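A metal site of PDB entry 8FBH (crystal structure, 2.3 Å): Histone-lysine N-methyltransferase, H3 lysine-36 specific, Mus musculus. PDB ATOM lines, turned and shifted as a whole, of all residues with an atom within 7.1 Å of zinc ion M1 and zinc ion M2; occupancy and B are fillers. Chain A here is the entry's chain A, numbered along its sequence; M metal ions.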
ATOM      1  N   ARG A  44      -9.640   9.172  -7.972  1.00  0.00           N
ATOM      2  CA  ARG A  44     -10.540  10.357  -7.934  1.00  0.00           C
ATOM      3  C   ARG A  44     -10.408  11.111  -9.240  1.00  0.00           C
ATOM      4  O   ARG A  44      -9.258  11.411  -9.644  1.00  0.00           O
ATOM      5  CB  ARG A  44     -10.213  11.279  -6.757  1.00  0.00           C
ATOM      6  CG  ARG A  44     -10.372  10.653  -5.380  1.00  0.00           C
ATOM      7  CD  ARG A  44      -9.815  11.604  -4.345  1.00  0.00           C
ATOM      8  NE  ARG A  44     -10.344  11.432  -3.000  1.00  0.00           N
ATOM      9  CZ  ARG A  44      -9.728  10.782  -2.020  1.00  0.00           C
ATOM     10  NH1 ARG A  44      -8.537  10.223  -2.228  1.00  0.00           N
ATOM     11  NH2 ARG A  44     -10.321  10.672  -0.844  1.00  0.00           N
ATOM     12  N   CYS A  45     -11.518  11.355  -9.924  1.00  0.00           N
ATOM     13  CA  CYS A  45     -11.526  11.953 -11.274  1.00  0.00           C
ATOM     14  C   CYS A  45     -11.393  13.473 -11.131  1.00  0.00           C
ATOM     15  O   CYS A  45     -11.271  13.935  -9.967  1.00  0.00           O
ATOM     16  CB  CYS A  45     -12.791  11.580 -12.048  1.00  0.00           C
ATOM     17  SG  CYS A  45     -14.281  12.385 -11.400  1.00  0.00           S
ATOM     18  N   ASN A  46     -11.441  14.189 -12.269  1.00  0.00           N
ATOM     19  CA  ASN A  46     -11.276  15.649 -12.390  1.00  0.00           C
ATOM     20  C   ASN A  46     -12.641  16.350 -12.403  1.00  0.00           C
ATOM     21  O   ASN A  46     -12.645  17.560 -12.489  1.00  0.00           O
ATOM     22  CB  ASN A  46     -10.508  16.012 -13.671  1.00  0.00           C
ATOM     23  CG  ASN A  46     -11.026  15.307 -14.906  1.00  0.00           C
ATOM     24  OD1 ASN A  46     -11.449  14.158 -14.824  1.00  0.00           O
ATOM     25  ND2 ASN A  46     -10.969  15.981 -16.047  1.00  0.00           N
ATOM     26  N   CYS A  47     -13.741  15.623 -12.298  1.00  0.00           N
ATOM     27  CA  CYS A  47     -15.127  16.204 -12.327  1.00  0.00           C
ATOM     28  C   CYS A  47     -15.445  16.881 -10.993  1.00  0.00           C
ATOM     29  O   CYS A  47     -14.848  16.505  -9.952  1.00  0.00           O
ATOM     30  CB  CYS A  47     -16.182  15.150 -12.657  1.00  0.00           C
ATOM     31  SG  CYS A  47     -15.932  14.303 -14.245  1.00  0.00           S
ATOM     32  N   LYS A  48     -16.371  17.851 -11.025  1.00  0.00           N
ATOM     33  CA  LYS A  48     -16.857  18.629  -9.837  1.00  0.00           C
ATOM     34  C   LYS A  48     -18.381  18.532  -9.745  1.00  0.00           C
ATOM     35  O   LYS A  48     -19.045  18.481 -10.814  1.00  0.00           O
ATOM     36  CB  LYS A  48     -16.453  20.109  -9.971  1.00  0.00           C
ATOM     37  CG  LYS A  48     -14.956  20.401 -10.084  1.00  0.00           C
ATOM     38  CD  LYS A  48     -14.107  19.853  -8.922  1.00  0.00           C
ATOM     39  CE  LYS A  48     -12.621  20.163  -9.032  1.00  0.00           C
ATOM     40  NZ  LYS A  48     -11.903  19.264  -9.978  1.00  0.00           N
ATOM     41  N   ASP A  51     -20.320  20.833 -12.110  1.00  0.00           N
ATOM     42  CA  ASP A  51     -20.256  20.594 -13.587  1.00  0.00           C
ATOM     43  C   ASP A  51     -21.693  20.303 -14.055  1.00  0.00           C
ATOM     44  O   ASP A  51     -22.541  20.055 -13.166  1.00  0.00           O
ATOM     45  CB  ASP A  51     -19.280  19.478 -13.974  1.00  0.00           C
ATOM     46  CG  ASP A  51     -17.791  19.806 -13.798  1.00  0.00           C
ATOM     47  OD1 ASP A  51     -17.443  20.974 -13.569  1.00  0.00           O
ATOM     48  OD2 ASP A  51     -16.975  18.876 -13.885  1.00  0.00           O
ATOM     49  N   ASN A  53     -22.905  17.819 -16.204  1.00  0.00           N
ATOM     50  CA  ASN A  53     -23.131  16.358 -16.110  1.00  0.00           C
ATOM     51  C   ASN A  53     -21.882  15.698 -15.547  1.00  0.00           C
ATOM     52  O   ASN A  53     -21.103  15.065 -16.276  1.00  0.00           O
ATOM     53  CB  ASN A  53     -23.501  15.744 -17.462  1.00  0.00           C
ATOM     54  CG  ASN A  53     -24.875  16.157 -17.922  1.00  0.00           C
ATOM     55  OD1 ASN A  53     -25.860  15.832 -17.269  1.00  0.00           O
ATOM     56  ND2 ASN A  53     -24.962  16.885 -19.025  1.00  0.00           N
ATOM     57  N   PRO A  54     -21.670  15.787 -14.220  1.00  0.00           N
ATOM     58  CA  PRO A  54     -20.495  15.203 -13.601  1.00  0.00           C
ATOM     59  C   PRO A  54     -20.313  13.726 -14.000  1.00  0.00           C
ATOM     60  O   PRO A  54     -21.243  12.938 -13.813  1.00  0.00           O
ATOM     61  CB  PRO A  54     -20.748  15.321 -12.089  1.00  0.00           C
ATOM     62  CG  PRO A  54     -21.858  16.322 -11.943  1.00  0.00           C
ATOM     63  CD  PRO A  54     -22.627  16.308 -13.243  1.00  0.00           C
ATOM     64  N   CYS A  55     -19.150  13.394 -14.588  1.00  0.00           N
ATOM     65  CA  CYS A  55     -18.712  12.017 -14.919  1.00  0.00           C
ATOM     66  C   CYS A  55     -19.614  11.418 -16.033  1.00  0.00           C
ATOM     67  O   CYS A  55     -19.614  10.190 -16.232  1.00  0.00           O
ATOM     68  CB  CYS A  55     -18.675  11.139 -13.652  1.00  0.00           C
ATOM     69  SG  CYS A  55     -17.727  11.842 -12.263  1.00  0.00           S
ATOM     70  N   GLY A  56     -20.286  12.255 -16.809  1.00  0.00           N
ATOM     71  CA  GLY A  56     -21.189  11.813 -17.890  1.00  0.00           C
ATOM     72  C   GLY A  56     -20.440  11.434 -19.168  1.00  0.00           C
ATOM     73  O   GLY A  56     -19.213  11.731 -19.253  1.00  0.00           O
ATOM     74  N   SER A  59     -18.624  14.351 -20.598  1.00  0.00           N
ATOM     75  CA  SER A  59     -17.737  15.129 -19.670  1.00  0.00           C
ATOM     76  C   SER A  59     -16.250  14.829 -19.970  1.00  0.00           C
ATOM     77  O   SER A  59     -15.958  13.940 -20.787  1.00  0.00           O
ATOM     78  CB  SER A  59     -18.050  14.837 -18.225  1.00  0.00           C
ATOM     79  OG  SER A  59     -17.642  13.508 -17.888  1.00  0.00           O
ATOM     80  N   GLU A  60     -15.368  15.529 -19.266  1.00  0.00           N
ATOM     81  CA  GLU A  60     -13.898  15.422 -19.375  1.00  0.00           C
ATOM     82  C   GLU A  60     -13.367  14.318 -18.446  1.00  0.00           C
ATOM     83  O   GLU A  60     -12.112  14.152 -18.337  1.00  0.00           O
ATOM     84  CB  GLU A  60     -13.290  16.787 -19.042  1.00  0.00           C
ATOM     85  CG  GLU A  60     -13.791  17.919 -19.938  1.00  0.00           C
ATOM     86  CD  GLU A  60     -13.353  19.328 -19.517  1.00  0.00           C
ATOM     87  OE1 GLU A  60     -13.522  20.258 -20.322  1.00  0.00           O
ATOM     88  OE2 GLU A  60     -12.815  19.480 -18.375  1.00  0.00           O
ATOM     89  N   CYS A  61     -14.277  13.559 -17.831  1.00  0.00           N
ATOM     90  CA  CYS A  61     -13.989  12.590 -16.715  1.00  0.00           C
ATOM     91  C   CYS A  61     -12.882  11.604 -17.091  1.00  0.00           C
ATOM     92  O   CYS A  61     -13.127  10.742 -17.951  1.00  0.00           O
ATOM     93  CB  CYS A  61     -15.229  11.773 -16.350  1.00  0.00           C
ATOM     94  SG  CYS A  61     -14.982  10.814 -14.846  1.00  0.00           S
ATOM     95  N   ILE A  62     -11.763  11.648 -16.356  1.00  0.00           N
ATOM     96  CA  ILE A  62     -10.585  10.755 -16.572  1.00  0.00           C
ATOM     97  C   ILE A  62     -10.939   9.312 -16.193  1.00  0.00           C
ATOM     98  O   ILE A  62     -10.332   8.413 -16.788  1.00  0.00           O
ATOM     99  CB  ILE A  62      -9.353  11.262 -15.827  1.00  0.00           C
ATOM    100  CG1 ILE A  62      -8.083  10.557 -16.304  1.00  0.00           C
ATOM    101  CG2 ILE A  62      -9.505  11.124 -14.318  1.00  0.00           C
ATOM    102  CD1 ILE A  62      -7.758  10.820 -17.754  1.00  0.00           C
ATOM    103  N   ASN A  63     -11.814   9.088 -15.208  1.00  0.00           N
ATOM    104  CA  ASN A  63     -12.203   7.704 -14.829  1.00  0.00           C
ATOM    105  C   ASN A  63     -12.873   7.036 -16.048  1.00  0.00           C
ATOM    106  O   ASN A  63     -12.424   5.948 -16.479  1.00  0.00           O
ATOM    107  CB  ASN A  63     -13.006   7.669 -13.517  1.00  0.00           C
ATOM    108  CG  ASN A  63     -12.126   7.761 -12.284  1.00  0.00           C
ATOM    109  OD1 ASN A  63     -10.887   7.760 -12.403  1.00  0.00           O
ATOM    110  ND2 ASN A  63     -12.729   7.883 -11.104  1.00  0.00           N
ATOM    111  N   ARG A  64     -13.900   7.683 -16.608  1.00  0.00           N
ATOM    112  CA  ARG A  64     -14.668   7.149 -17.751  1.00  0.00           C
ATOM    113  C   ARG A  64     -13.704   7.016 -18.945  1.00  0.00           C
ATOM    114  O   ARG A  64     -13.742   5.976 -19.601  1.00  0.00           O
ATOM    115  CB  ARG A  64     -15.899   8.053 -17.966  1.00  0.00           C
ATOM    116  CG  ARG A  64     -16.600   7.917 -19.298  1.00  0.00           C
ATOM    117  CD  ARG A  64     -17.761   8.884 -19.427  1.00  0.00           C
ATOM    118  NE  ARG A  64     -18.864   8.565 -18.533  1.00  0.00           N
ATOM    119  CZ  ARG A  64     -19.704   7.554 -18.698  1.00  0.00           C
ATOM    120  NH1 ARG A  64     -19.569   6.736 -19.728  1.00  0.00           N
ATOM    121  NH2 ARG A  64     -20.687   7.350 -17.835  1.00  0.00           N
ATOM    122  N   GLU A  69     -14.970   2.808 -13.394  1.00  0.00           N
ATOM    123  CA  GLU A  69     -16.208   3.261 -12.713  1.00  0.00           C
ATOM    124  C   GLU A  69     -15.821   4.007 -11.413  1.00  0.00           C
ATOM    125  O   GLU A  69     -14.904   3.563 -10.706  1.00  0.00           O
ATOM    126  CB  GLU A  69     -17.111   2.053 -12.477  1.00  0.00           C
ATOM    127  CG  GLU A  69     -18.320   2.383 -11.633  1.00  0.00           C
ATOM    128  CD  GLU A  69     -19.564   1.563 -11.927  1.00  0.00           C
ATOM    129  OE1 GLU A  69     -20.243   1.152 -10.952  1.00  0.00           O
ATOM    130  OE2 GLU A  69     -19.892   1.394 -13.116  1.00  0.00           O
ATOM    131  N   CYS A  70     -16.499   5.098 -11.119  1.00  0.00           N
ATOM    132  CA  CYS A  70     -16.344   5.841  -9.846  1.00  0.00           C
ATOM    133  C   CYS A  70     -16.930   5.033  -8.681  1.00  0.00           C
ATOM    134  O   CYS A  70     -17.916   4.294  -8.909  1.00  0.00           O
ATOM    135  CB  CYS A  70     -17.023   7.202  -9.928  1.00  0.00           C
ATOM    136  SG  CYS A  70     -16.211   8.329 -11.080  1.00  0.00           S
ATOM    137  N   HIS A  71     -16.360   5.191  -7.499  1.00  0.00           N
ATOM    138  CA  HIS A  71     -16.971   4.749  -6.219  1.00  0.00           C
ATOM    139  C   HIS A  71     -17.741   5.929  -5.613  1.00  0.00           C
ATOM    140  O   HIS A  71     -17.215   7.033  -5.546  1.00  0.00           O
ATOM    141  CB  HIS A  71     -15.918   4.147  -5.270  1.00  0.00           C
ATOM    142  CG  HIS A  71     -16.569   3.338  -4.193  1.00  0.00           C
ATOM    143  ND1 HIS A  71     -17.227   3.930  -3.133  1.00  0.00           N
ATOM    144  CD2 HIS A  71     -16.827   2.008  -4.107  1.00  0.00           C
ATOM    145  CE1 HIS A  71     -17.796   3.005  -2.391  1.00  0.00           C
ATOM    146  NE2 HIS A  71     -17.556   1.811  -2.966  1.00  0.00           N
ATOM    147  N   VAL A  74     -16.162   8.082  -2.907  1.00  0.00           N
ATOM    148  CA  VAL A  74     -14.797   8.588  -3.295  1.00  0.00           C
ATOM    149  C   VAL A  74     -14.902   9.693  -4.352  1.00  0.00           C
ATOM    150  O   VAL A  74     -14.052  10.605  -4.333  1.00  0.00           O
ATOM    151  CB  VAL A  74     -13.903   7.432  -3.794  1.00  0.00           C
ATOM    152  CG1 VAL A  74     -12.707   7.914  -4.579  1.00  0.00           C
ATOM    153  CG2 VAL A  74     -13.440   6.553  -2.646  1.00  0.00           C
ATOM    154  N   CYS A  75     -15.847   9.601  -5.287  1.00  0.00           N
ATOM    155  CA  CYS A  75     -15.983  10.559  -6.394  1.00  0.00           C
ATOM    156  C   CYS A  75     -16.310  11.951  -5.836  1.00  0.00           C
ATOM    157  O   CYS A  75     -17.271  12.115  -5.113  1.00  0.00           O
ATOM    158  CB  CYS A  75     -17.056  10.154  -7.398  1.00  0.00           C
ATOM    159  SG  CYS A  75     -17.153  11.319  -8.781  1.00  0.00           S
ATOM    160  N   PRO A  76     -15.531  12.989  -6.210  1.00  0.00           N
ATOM    161  CA  PRO A  76     -15.780  14.350  -5.742  1.00  0.00           C
ATOM    162  C   PRO A  76     -17.134  14.918  -6.150  1.00  0.00           C
ATOM    163  O   PRO A  76     -17.524  15.883  -5.549  1.00  0.00           O
ATOM    164  CB  PRO A  76     -14.701  15.196  -6.446  1.00  0.00           C
ATOM    165  CG  PRO A  76     -13.610  14.199  -6.762  1.00  0.00           C
ATOM    166  CD  PRO A  76     -14.318  12.887  -7.021  1.00  0.00           C
ATOM    167  N   ALA A  77     -17.756  14.380  -7.191  1.00  0.00           N
ATOM    168  CA  ALA A  77     -19.100  14.787  -7.664  1.00  0.00           C
ATOM    169  C   ALA A  77     -20.200  14.184  -6.771  1.00  0.00           C
ATOM    170  O   ALA A  77     -21.348  14.658  -6.852  1.00  0.00           O
ATOM    171  CB  ALA A  77     -19.271  14.382  -9.100  1.00  0.00           C
ATOM    172  N   GLY A  78     -19.846  13.229  -5.911  1.00  0.00           N
ATOM    173  CA  GLY A  78     -20.777  12.554  -4.988  1.00  0.00           C
ATOM    174  C   GLY A  78     -21.923  11.859  -5.726  1.00  0.00           C
ATOM    175  O   GLY A  78     -21.663  11.216  -6.778  1.00  0.00           O
ATOM    176  N   ARG A  80     -24.074  13.048  -7.542  1.00  0.00           N
ATOM    177  CA  ARG A  80     -24.283  13.649  -8.878  1.00  0.00           C
ATOM    178  C   ARG A  80     -23.471  12.879  -9.954  1.00  0.00           C
ATOM    179  O   ARG A  80     -23.714  13.117 -11.180  1.00  0.00           O
ATOM    180  CB  ARG A  80     -23.993  15.154  -8.829  1.00  0.00           C
ATOM    181  CG  ARG A  80     -25.084  15.943  -8.077  1.00  0.00           C
ATOM    182  CD  ARG A  80     -25.065  17.464  -8.200  1.00  0.00           C
ATOM    183  NE  ARG A  80     -24.489  17.988  -9.436  1.00  0.00           N
ATOM    184  CZ  ARG A  80     -25.089  18.054 -10.644  1.00  0.00           C
ATOM    185  NH1 ARG A  80     -24.432  18.573 -11.673  1.00  0.00           N
ATOM    186  NH2 ARG A  80     -26.317  17.603 -10.814  1.00  0.00           N
ATOM    187  N   CYS A  81     -22.626  11.913  -9.521  1.00  0.00           N
ATOM    188  CA  CYS A  81     -21.773  11.032 -10.382  1.00  0.00           C
ATOM    189  C   CYS A  81     -22.623  10.238 -11.386  1.00  0.00           C
ATOM    190  O   CYS A  81     -23.396   9.413 -10.941  1.00  0.00           O
ATOM    191  CB  CYS A  81     -20.985  10.042  -9.544  1.00  0.00           C
ATOM    192  SG  CYS A  81     -19.750   9.107 -10.468  1.00  0.00           S
ATOM    193  N   GLN A  82     -22.416  10.441 -12.696  1.00  0.00           N
ATOM    194  CA  GLN A  82     -23.106   9.705 -13.803  1.00  0.00           C
ATOM    195  C   GLN A  82     -22.207   8.576 -14.349  1.00  0.00           C
ATOM    196  O   GLN A  82     -22.396   8.191 -15.518  1.00  0.00           O
ATOM    197  CB  GLN A  82     -23.456  10.697 -14.912  1.00  0.00           C
ATOM    198  CG  GLN A  82     -24.495  11.736 -14.512  1.00  0.00           C
ATOM    199  CD  GLN A  82     -24.793  12.686 -15.650  1.00  0.00           C
ATOM    200  OE1 GLN A  82     -24.480  12.429 -16.811  1.00  0.00           O
ATOM    201  NE2 GLN A  82     -25.383  13.829 -15.314  1.00  0.00           N
ATOM    202  N   ASN A  83     -21.251   8.081 -13.551  1.00  0.00           N
ATOM    203  CA  ASN A  83     -20.261   7.049 -13.947  1.00  0.00           C
ATOM    204  C   ASN A  83     -20.355   5.862 -12.980  1.00  0.00           C
ATOM    205  O   ASN A  83     -19.290   5.440 -12.482  1.00  0.00           O
ATOM    206  CB  ASN A  83     -18.844   7.611 -14.015  1.00  0.00           C
ATOM    207  CG  ASN A  83     -17.852   6.643 -14.635  1.00  0.00           C
ATOM    208  OD1 ASN A  83     -18.257   5.812 -15.440  1.00  0.00           O
ATOM    209  ND2 ASN A  83     -16.595   6.732 -14.267  1.00  0.00           N
ATOM    210  N   GLN A  84     -21.564   5.337 -12.727  1.00  0.00           N
ATOM    211  CA  GLN A  84     -21.794   4.179 -11.818  1.00  0.00           C
ATOM    212  C   GLN A  84     -22.739   3.166 -12.494  1.00  0.00           C
ATOM    213  O   GLN A  84     -23.523   2.521 -11.769  1.00  0.00           O
ATOM    214  CB  GLN A  84     -22.338   4.666 -10.477  1.00  0.00           C
ATOM    215  CG  GLN A  84     -21.291   5.401  -9.657  1.00  0.00           C
ATOM    216  CD  GLN A  84     -21.853   6.132  -8.461  1.00  0.00           C
ATOM    217  OE1 GLN A  84     -21.512   7.285  -8.203  1.00  0.00           O
ATOM    218  NE2 GLN A  84     -22.681   5.456  -7.687  1.00  0.00           N
HETATM  219 ZN    ZN M   1     -17.638  10.137 -10.736  1.00  0.00          ZN
HETATM  220 ZN    ZN M   2     -15.662  12.184 -13.174  1.00  0.00          ZN
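Zinc ion M2 is bound by SG of Cys 45, SG of Cys 61, SG of Cys 55 and SG of Cys 47.
Within 4 Å of zinc ion M2: Cys 45, Cys 47, Cys 55 and Cys 61. The nearest printed residue that does not touch zinc ion M2 is Cys 70 (4.4 Å).
Four residues have an atom within 4 Å of zinc ion M1: Cys 55, Cys 70, Cys 75 and Cys 81.
The side-chain sulfur of Cys 75 sits close to the backbone NH of Ala 77 (3.5 Å). The guanidinium group (NE) of Arg 64 lies within hydrogen-bond range of the backbone carbonyl oxygen (O) of Cys 55 (2.9 Å). N of Cys 61 sits close to OG of Ser 59 (3.4 Å). The backbone NH (N) of Cys 70 is in hydrogen-bond range of the backbone carbonyl oxygen (O) of Asn 83. N of Asn 83 lies close to SG of Cys 81 (3.6 Å). The side-chain sulfur (SG) of Cys 61 lies close to the backbone NH (N) of Arg 64 (3.8 Å). The side-chain sulfur (SG) of Cys 70 sits close to the side-chain amide nitrogen (ND2) of Asn 63, at 3.5 Å. SG of Cys 61 lies close to N of Asn 63, 3.6 Å away.
Zinc ion M1 is bound by SG of Cys 55, 2.3 Å away. Zinc ion M1 is bound by SG of Cys 70 (2.3 Å). SG of Cys 75 is bound to zinc ion M1 (2.3 Å). The side-chain sulfur (SG) of Cys 81 binds zinc ion M1.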
